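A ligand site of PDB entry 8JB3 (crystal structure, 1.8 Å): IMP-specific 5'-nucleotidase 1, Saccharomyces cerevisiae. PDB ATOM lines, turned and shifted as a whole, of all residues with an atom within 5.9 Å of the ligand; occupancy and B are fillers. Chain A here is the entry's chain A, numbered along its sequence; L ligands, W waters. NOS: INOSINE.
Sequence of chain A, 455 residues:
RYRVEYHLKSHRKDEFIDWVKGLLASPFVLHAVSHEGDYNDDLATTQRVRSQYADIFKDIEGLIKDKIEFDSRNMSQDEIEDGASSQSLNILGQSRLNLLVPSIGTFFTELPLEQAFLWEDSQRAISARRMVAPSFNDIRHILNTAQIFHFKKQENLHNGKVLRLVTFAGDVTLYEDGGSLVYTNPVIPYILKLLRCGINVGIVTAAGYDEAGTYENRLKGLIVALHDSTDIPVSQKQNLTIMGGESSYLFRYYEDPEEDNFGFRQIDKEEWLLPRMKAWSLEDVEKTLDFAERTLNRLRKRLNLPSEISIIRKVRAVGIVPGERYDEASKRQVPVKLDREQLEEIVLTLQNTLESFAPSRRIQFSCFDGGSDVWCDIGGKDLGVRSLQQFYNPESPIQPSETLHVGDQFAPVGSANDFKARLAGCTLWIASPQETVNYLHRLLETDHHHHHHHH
OD1 of Asp 14 is in hydrogen-bond range of N1 of the ligand (3.0 Å). An oxygen (O2') of the ligand lies within hydrogen-bond range of the side-chain hydroxyl of Thr 427, 2.7 Å away. OE1 of Gln 147 sits at hydrogen-bond distance from O3' of the ligand. A nitrogen (N7) of the ligand lies within hydrogen-bond range of the backbone NH (N) of Gly 105 (3.1 Å). An oxygen (O3') of the ligand lies within hydrogen-bond range of the backbone NH (N) of Thr 427 (3.1 Å).
OD2 of Asp 14 sits at hydrogen-bond distance from N of Ile 17, at 3.0 Å. The side-chain carboxylate of Asp 14 lies within salt-bridge range of the guanidinium group of Arg 422, 2.8 Å away. The side-chain carboxylate (OD2) of Asp 14 lies close to the backbone NH (N) of Phe 16, at 3.3 Å. SG of Cys 426 sits close to OE1 of Gln 147 (3.5 Å).
N1 of the ligand lies close to NH1 of Arg 422 (3.4 Å). Merely in contact with the ligand: Phe 16, Ile 104, Thr 106, Phe 107, Leu 111, Leu 143 and Cys 426. Hydrophobic or aromatic side chains that line the ligand: Phe 16, Ile 104, Phe 107, Leu 111 and Leu 143. Within 4 Å of the ligand: Asp 14, Phe 16, Ile 104, Gly 105, Thr 106, Phe 107, Leu 111, Leu 143, Gln 147, Arg 422, Cys 426 and Thr 427. The nearest printed residue that does not touch the ligand is Ser 103 (4.2 Å).
Water W5 lies within hydrogen-bond range of O6 of the ligand, N of Phe 16, OG of Ser 103, N of Glu 15 and OD2 of Asp 14. Water W3 lies within hydrogen-bond range of an oxygen (O2') of the ligand (2.8 Å), the backbone carbonyl oxygen (O) of Gly 425 (2.8 Å) and the backbone carbonyl oxygen (O) of Thr 106 (3.3 Å). Water W4 lies within hydrogen-bond range of the guanidinium group (NH1) of Arg 422, an oxygen (O6) of the ligand and the backbone NH (N) of Gly 105. Water W6 lies within hydrogen-bond range of OD1 of Asn 144 (2.7 Å), O of Thr 427 (2.7 Å) and O5' of the ligand (3.3 Å). Water W1 bridges O3' of the ligand (3.3 Å) and SG of Cys 426 (3.8 Å).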
ATOM      1  N   ASP A  14      -2.873  23.125  12.004  1.00  0.00           N
ATOM      2  CA  ASP A  14      -1.478  23.209  12.448  1.00  0.00           C
ATOM      3  C   ASP A  14      -0.508  23.054  11.261  1.00  0.00           C
ATOM      4  O   ASP A  14      -0.385  21.957  10.676  1.00  0.00           O
ATOM      5  CB  ASP A  14      -1.210  22.132  13.502  1.00  0.00           C
ATOM      6  CG  ASP A  14       0.073  22.376  14.277  1.00  0.00           C
ATOM      7  OD1 ASP A  14      -0.008  22.799  15.463  1.00  0.00           O
ATOM      8  OD2 ASP A  14       1.155  22.117  13.738  1.00  0.00           O
ATOM      9  N   GLU A  15       0.171  24.138  10.885  1.00  0.00           N
ATOM     10  CA  GLU A  15       0.992  24.153   9.667  1.00  0.00           C
ATOM     11  C   GLU A  15       2.124  23.153   9.802  1.00  0.00           C
ATOM     12  O   GLU A  15       2.471  22.490   8.846  1.00  0.00           O
ATOM     13  CB  GLU A  15       1.566  25.554   9.376  1.00  0.00           C
ATOM     14  CG  GLU A  15       2.342  25.567   8.049  1.00  0.00           C
ATOM     15  CD  GLU A  15       3.166  26.832   7.779  1.00  0.00           C
ATOM     16  OE1 GLU A  15       3.367  27.665   8.681  1.00  0.00           O
ATOM     17  OE2 GLU A  15       3.618  26.990   6.621  1.00  0.00           O
ATOM     18  N   PHE A  16       2.699  23.063  10.999  1.00  0.00           N
ATOM     19  CA  PHE A  16       3.825  22.147  11.266  1.00  0.00           C
ATOM     20  C   PHE A  16       3.411  20.689  11.054  1.00  0.00           C
ATOM     21  O   PHE A  16       4.112  19.937  10.386  1.00  0.00           O
ATOM     22  CB  PHE A  16       4.356  22.321  12.685  1.00  0.00           C
ATOM     23  CG  PHE A  16       5.522  21.406  13.028  1.00  0.00           C
ATOM     24  CD1 PHE A  16       6.598  21.268  12.160  1.00  0.00           C
ATOM     25  CD2 PHE A  16       5.542  20.718  14.228  1.00  0.00           C
ATOM     26  CE1 PHE A  16       7.679  20.440  12.490  1.00  0.00           C
ATOM     27  CE2 PHE A  16       6.615  19.888  14.579  1.00  0.00           C
ATOM     28  CZ  PHE A  16       7.678  19.745  13.701  1.00  0.00           C
ATOM     29  N   ILE A  17       2.298  20.281  11.651  1.00  0.00           N
ATOM     30  CA  ILE A  17       1.827  18.897  11.464  1.00  0.00           C
ATOM     31  C   ILE A  17       1.486  18.631   9.995  1.00  0.00           C
ATOM     32  O   ILE A  17       1.901  17.632   9.417  1.00  0.00           O
ATOM     33  CB  ILE A  17       0.621  18.593  12.368  1.00  0.00           C
ATOM     34  CG1 ILE A  17       1.087  18.572  13.839  1.00  0.00           C
ATOM     35  CG2 ILE A  17      -0.008  17.227  11.953  1.00  0.00           C
ATOM     36  CD1 ILE A  17      -0.022  18.394  14.840  1.00  0.00           C
ATOM     37  N   VAL A 101       8.756  26.353   7.978  1.00  0.00           N
ATOM     38  CA  VAL A 101       7.407  26.391   8.559  1.00  0.00           C
ATOM     39  C   VAL A 101       7.220  27.714   9.302  1.00  0.00           C
ATOM     40  O   VAL A 101       7.452  27.795  10.492  1.00  0.00           O
ATOM     41  CB  VAL A 101       7.174  25.191   9.532  1.00  0.00           C
ATOM     42  CG1 VAL A 101       5.732  25.159  10.052  1.00  0.00           C
ATOM     43  CG2 VAL A 101       7.550  23.882   8.864  1.00  0.00           C
ATOM     44  N   SER A 103       4.945  29.535  10.560  1.00  0.00           N
ATOM     45  CA  SER A 103       4.045  29.714  11.693  1.00  0.00           C
ATOM     46  C   SER A 103       4.471  28.864  12.873  1.00  0.00           C
ATOM     47  O   SER A 103       3.790  28.826  13.901  1.00  0.00           O
ATOM     48  CB  SER A 103       2.610  29.378  11.299  1.00  0.00           C
ATOM     49  OG  SER A 103       2.442  27.969  11.178  1.00  0.00           O
ATOM     50  N   ILE A 104       5.603  28.189  12.754  1.00  0.00           N
ATOM     51  CA  ILE A 104       6.002  27.312  13.835  1.00  0.00           C
ATOM     52  C   ILE A 104       6.231  28.090  15.153  1.00  0.00           C
ATOM     53  O   ILE A 104       6.637  29.262  15.145  1.00  0.00           O
ATOM     54  CB  ILE A 104       7.255  26.496  13.444  1.00  0.00           C
ATOM     55  CG1 ILE A 104       7.356  25.250  14.324  1.00  0.00           C
ATOM     56  CG2 ILE A 104       8.531  27.385  13.431  1.00  0.00           C
ATOM     57  CD1 ILE A 104       8.015  24.080  13.704  1.00  0.00           C
ATOM     58  N   GLY A 105       5.924  27.443  16.280  1.00  0.00           N
ATOM     59  CA  GLY A 105       6.119  28.030  17.599  1.00  0.00           C
ATOM     60  C   GLY A 105       7.512  27.711  18.121  1.00  0.00           C
ATOM     61  O   GLY A 105       8.420  27.342  17.358  1.00  0.00           O
ATOM     62  N   THR A 106       7.701  27.851  19.425  1.00  0.00           N
ATOM     63  CA  THR A 106       8.985  27.642  20.062  1.00  0.00           C
ATOM     64  C   THR A 106       9.071  26.216  20.607  1.00  0.00           C
ATOM     65  O   THR A 106       8.100  25.710  21.131  1.00  0.00           O
ATOM     66  CB  THR A 106       9.194  28.659  21.245  1.00  0.00           C
ATOM     67  OG1 THR A 106       9.327  29.969  20.701  1.00  0.00           O
ATOM     68  CG2 THR A 106      10.434  28.328  22.039  1.00  0.00           C
ATOM     69  N   PHE A 107      10.232  25.591  20.466  1.00  0.00           N
ATOM     70  CA  PHE A 107      10.449  24.309  21.126  1.00  0.00           C
ATOM     71  C   PHE A 107      11.268  24.558  22.381  1.00  0.00           C
ATOM     72  O   PHE A 107      12.388  25.060  22.280  1.00  0.00           O
ATOM     73  CB  PHE A 107      11.148  23.321  20.204  1.00  0.00           C
ATOM     74  CG  PHE A 107      10.339  22.960  18.993  1.00  0.00           C
ATOM     75  CD1 PHE A 107       9.353  21.983  19.090  1.00  0.00           C
ATOM     76  CD2 PHE A 107      10.534  23.609  17.782  1.00  0.00           C
ATOM     77  CE1 PHE A 107       8.590  21.622  17.978  1.00  0.00           C
ATOM     78  CE2 PHE A 107       9.766  23.275  16.662  1.00  0.00           C
ATOM     79  CZ  PHE A 107       8.784  22.274  16.777  1.00  0.00           C
ATOM     80  N   LEU A 111      12.866  16.998  20.952  1.00  0.00           N
ATOM     81  CA  LEU A 111      11.827  15.976  20.785  1.00  0.00           C
ATOM     82  C   LEU A 111      12.415  14.725  20.129  1.00  0.00           C
ATOM     83  O   LEU A 111      12.890  14.778  18.984  1.00  0.00           O
ATOM     84  CB  LEU A 111      10.664  16.505  19.939  1.00  0.00           C
ATOM     85  CG  LEU A 111       9.871  17.656  20.585  1.00  0.00           C
ATOM     86  CD1 LEU A 111       8.841  18.195  19.611  1.00  0.00           C
ATOM     87  CD2 LEU A 111       9.171  17.141  21.868  1.00  0.00           C
ATOM     88  N   LEU A 143       4.024  13.444  17.910  1.00  0.00           N
ATOM     89  CA  LEU A 143       4.537  14.617  18.603  1.00  0.00           C
ATOM     90  C   LEU A 143       4.272  14.541  20.130  1.00  0.00           C
ATOM     91  O   LEU A 143       5.173  14.840  20.928  1.00  0.00           O
ATOM     92  CB  LEU A 143       3.930  15.902  18.001  1.00  0.00           C
ATOM     93  CG  LEU A 143       4.381  16.359  16.577  1.00  0.00           C
ATOM     94  CD1 LEU A 143       3.720  17.688  16.261  1.00  0.00           C
ATOM     95  CD2 LEU A 143       5.855  16.550  16.578  1.00  0.00           C
ATOM     96  N   ASN A 144       3.056  14.155  20.534  1.00  0.00           N
ATOM     97  CA  ASN A 144       2.730  14.029  21.976  1.00  0.00           C
ATOM     98  C   ASN A 144       3.630  12.998  22.655  1.00  0.00           C
ATOM     99  O   ASN A 144       4.192  13.244  23.710  1.00  0.00           O
ATOM    100  CB  ASN A 144       1.283  13.614  22.201  1.00  0.00           C
ATOM    101  CG  ASN A 144       0.308  14.709  21.884  1.00  0.00           C
ATOM    102  OD1 ASN A 144       0.670  15.887  21.871  1.00  0.00           O
ATOM    103  ND2 ASN A 144      -0.942  14.317  21.586  1.00  0.00           N
ATOM    104  N   GLN A 147       7.050  14.283  23.154  1.00  0.00           N
ATOM    105  CA  GLN A 147       7.156  15.257  24.246  1.00  0.00           C
ATOM    106  C   GLN A 147       7.171  14.516  25.587  1.00  0.00           C
ATOM    107  O   GLN A 147       7.909  14.912  26.487  1.00  0.00           O
ATOM    108  CB  GLN A 147       6.018  16.281  24.187  1.00  0.00           C
ATOM    109  CG  GLN A 147       6.157  17.419  25.213  1.00  0.00           C
ATOM    110  CD  GLN A 147       7.367  18.295  24.925  1.00  0.00           C
ATOM    111  OE1 GLN A 147       7.298  19.271  24.149  1.00  0.00           O
ATOM    112  NE2 GLN A 147       8.495  17.946  25.547  1.00  0.00           N
ATOM    113  N   LEU A 404       4.395  21.460  31.250  1.00  0.00           N
ATOM    114  CA  LEU A 404       3.627  20.753  30.229  1.00  0.00           C
ATOM    115  C   LEU A 404       2.143  21.065  30.382  1.00  0.00           C
ATOM    116  O   LEU A 404       1.532  20.647  31.382  1.00  0.00           O
ATOM    117  CB  LEU A 404       3.852  19.247  30.328  1.00  0.00           C
ATOM    118  CG  LEU A 404       3.184  18.373  29.251  1.00  0.00           C
ATOM    119  CD1 LEU A 404       3.785  18.651  27.830  1.00  0.00           C
ATOM    120  CD2 LEU A 404       3.252  16.892  29.601  1.00  0.00           C
ATOM    121  N   PHE A 410      -6.016  23.620  20.296  1.00  0.00           N
ATOM    122  CA  PHE A 410      -4.702  24.072  19.840  1.00  0.00           C
ATOM    123  C   PHE A 410      -4.648  24.589  18.415  1.00  0.00           C
ATOM    124  O   PHE A 410      -3.574  24.862  17.885  1.00  0.00           O
ATOM    125  CB  PHE A 410      -3.661  22.960  20.021  1.00  0.00           C
ATOM    126  CG  PHE A 410      -3.073  22.915  21.405  1.00  0.00           C
ATOM    127  CD1 PHE A 410      -2.105  23.835  21.784  1.00  0.00           C
ATOM    128  CD2 PHE A 410      -3.502  21.962  22.350  1.00  0.00           C
ATOM    129  CE1 PHE A 410      -1.556  23.798  23.068  1.00  0.00           C
ATOM    130  CE2 PHE A 410      -2.975  21.921  23.655  1.00  0.00           C
ATOM    131  CZ  PHE A 410      -1.986  22.855  24.000  1.00  0.00           C
ATOM    132  N   ARG A 422       1.483  27.384  24.130  1.00  0.00           N
ATOM    133  CA  ARG A 422       2.762  27.087  23.473  1.00  0.00           C
ATOM    134  C   ARG A 422       3.793  28.193  23.698  1.00  0.00           C
ATOM    135  O   ARG A 422       4.984  27.962  23.537  1.00  0.00           O
ATOM    136  CB  ARG A 422       2.552  26.905  21.969  1.00  0.00           C
ATOM    137  CG  ARG A 422       1.759  25.651  21.611  1.00  0.00           C
ATOM    138  CD  ARG A 422       1.883  25.395  20.117  1.00  0.00           C
ATOM    139  NE  ARG A 422       1.109  24.202  19.752  1.00  0.00           N
ATOM    140  CZ  ARG A 422       0.548  24.029  18.571  1.00  0.00           C
ATOM    141  NH1 ARG A 422       0.719  24.972  17.669  1.00  0.00           N
ATOM    142  NH2 ARG A 422      -0.166  22.927  18.300  1.00  0.00           N
ATOM    143  N   GLY A 425       5.369  27.191  27.505  1.00  0.00           N
ATOM    144  CA  GLY A 425       5.852  25.872  27.938  1.00  0.00           C
ATOM    145  C   GLY A 425       5.597  24.790  26.885  1.00  0.00           C
ATOM    146  O   GLY A 425       5.046  25.098  25.824  1.00  0.00           O
ATOM    147  N   CYS A 426       6.028  23.564  27.161  1.00  0.00           N
ATOM    148  CA  CYS A 426       5.663  22.393  26.355  1.00  0.00           C
ATOM    149  C   CYS A 426       4.159  22.148  26.409  1.00  0.00           C
ATOM    150  O   CYS A 426       3.483  22.537  27.364  1.00  0.00           O
ATOM    151  CB  CYS A 426       6.396  21.150  26.841  1.00  0.00           C
ATOM    152  SG  CYS A 426       8.158  21.380  26.856  1.00  0.00           S
ATOM    153  N   THR A 427       3.619  21.493  25.372  1.00  0.00           N
ATOM    154  CA  THR A 427       2.202  21.162  25.397  1.00  0.00           C
ATOM    155  C   THR A 427       1.993  19.734  24.943  1.00  0.00           C
ATOM    156  O   THR A 427       2.881  19.153  24.304  1.00  0.00           O
ATOM    157  CB  THR A 427       1.383  22.103  24.533  1.00  0.00           C
ATOM    158  OG1 THR A 427       1.739  21.937  23.148  1.00  0.00           O
ATOM    159  CG2 THR A 427       1.661  23.557  24.943  1.00  0.00           C
ATOM    160  N   LEU A 428       0.842  19.177  25.319  1.00  0.00           N
ATOM    161  CA  LEU A 428       0.305  17.935  24.802  1.00  0.00           C
ATOM    162  C   LEU A 428      -1.034  18.257  24.190  1.00  0.00           C
ATOM    163  O   LEU A 428      -1.890  18.858  24.857  1.00  0.00           O
ATOM    164  CB  LEU A 428       0.132  16.902  25.919  1.00  0.00           C
ATOM    165  CG  LEU A 428       0.753  15.531  25.804  1.00  0.00           C
ATOM    166  CD1 LEU A 428       2.259  15.645  25.517  1.00  0.00           C
ATOM    167  CD2 LEU A 428       0.460  14.750  27.119  1.00  0.00           C
ATOM    168  N   TRP A 429      -1.236  17.869  22.937  1.00  0.00           N
ATOM    169  CA  TRP A 429      -2.477  18.186  22.240  1.00  0.00           C
ATOM    170  C   TRP A 429      -3.361  16.956  22.243  1.00  0.00           C
ATOM    171  O   TRP A 429      -3.089  16.002  21.493  1.00  0.00           O
ATOM    172  CB  TRP A 429      -2.193  18.610  20.790  1.00  0.00           C
ATOM    173  CG  TRP A 429      -3.389  19.071  19.982  1.00  0.00           C
ATOM    174  CD1 TRP A 429      -4.741  18.974  20.299  1.00  0.00           C
ATOM    175  CD2 TRP A 429      -3.324  19.702  18.702  1.00  0.00           C
ATOM    176  NE1 TRP A 429      -5.501  19.543  19.288  1.00  0.00           N
ATOM    177  CE2 TRP A 429      -4.646  19.996  18.309  1.00  0.00           C
ATOM    178  CE3 TRP A 429      -2.265  20.100  17.883  1.00  0.00           C
ATOM    179  CZ2 TRP A 429      -4.927  20.665  17.102  1.00  0.00           C
ATOM    180  CZ3 TRP A 429      -2.547  20.731  16.677  1.00  0.00           C
ATOM    181  CH2 TRP A 429      -3.861  21.012  16.309  1.00  0.00           C
HETATM  182  N9  NOS L   1       5.544  23.091  19.314  1.00  0.00           N
HETATM  183  C4  NOS L   1       4.584  22.808  18.328  1.00  0.00           C
HETATM  184  N3  NOS L   1       3.698  21.748  18.061  1.00  0.00           N
HETATM  185  C2  NOS L   1       2.863  21.780  16.972  1.00  0.00           C
HETATM  186  N1  NOS L   1       2.874  22.849  16.144  1.00  0.00           N
HETATM  187  C6  NOS L   1       3.738  23.876  16.367  1.00  0.00           C
HETATM  188  O6  NOS L   1       3.635  24.928  15.418  1.00  0.00           O
HETATM  189  C5  NOS L   1       4.572  23.850  17.474  1.00  0.00           C
HETATM  190  N7  NOS L   1       5.464  24.786  17.894  1.00  0.00           N
HETATM  191  C8  NOS L   1       6.033  24.310  19.007  1.00  0.00           C
HETATM  192  C5' NOS L   1       5.220  18.684  20.328  1.00  0.00           C
HETATM  193  O5' NOS L   1       4.065  19.094  19.601  1.00  0.00           O
HETATM  194  C4' NOS L   1       5.858  19.885  21.002  1.00  0.00           C
HETATM  195  O4' NOS L   1       6.182  20.888  19.981  1.00  0.00           O
HETATM  196  C1' NOS L   1       5.698  22.125  20.419  1.00  0.00           C
HETATM  197  C2' NOS L   1       4.437  21.789  21.223  1.00  0.00           C
HETATM  198  O2' NOS L   1       4.022  22.856  22.043  1.00  0.00           O
HETATM  199  C3' NOS L   1       4.917  20.576  22.001  1.00  0.00           C
HETATM  200  O3' NOS L   1       5.660  21.010  23.143  1.00  0.00           O
HETATM  201  O   HOH W   1       8.260  23.057  23.501  1.00  0.00           O
HETATM  202  O   HOH W   2       1.418  19.115  19.014  1.00  0.00           O
HETATM  203  O   HOH W   3       5.971  24.364  23.297  1.00  0.00           O
HETATM  204  O   HOH W   4       2.575  27.172  17.214  1.00  0.00           O
HETATM  205  O   HOH W   5       2.505  25.272  13.133  1.00  0.00           O
HETATM  206  O   HOH W   6       2.873  17.442  22.161  1.00  0.00           O
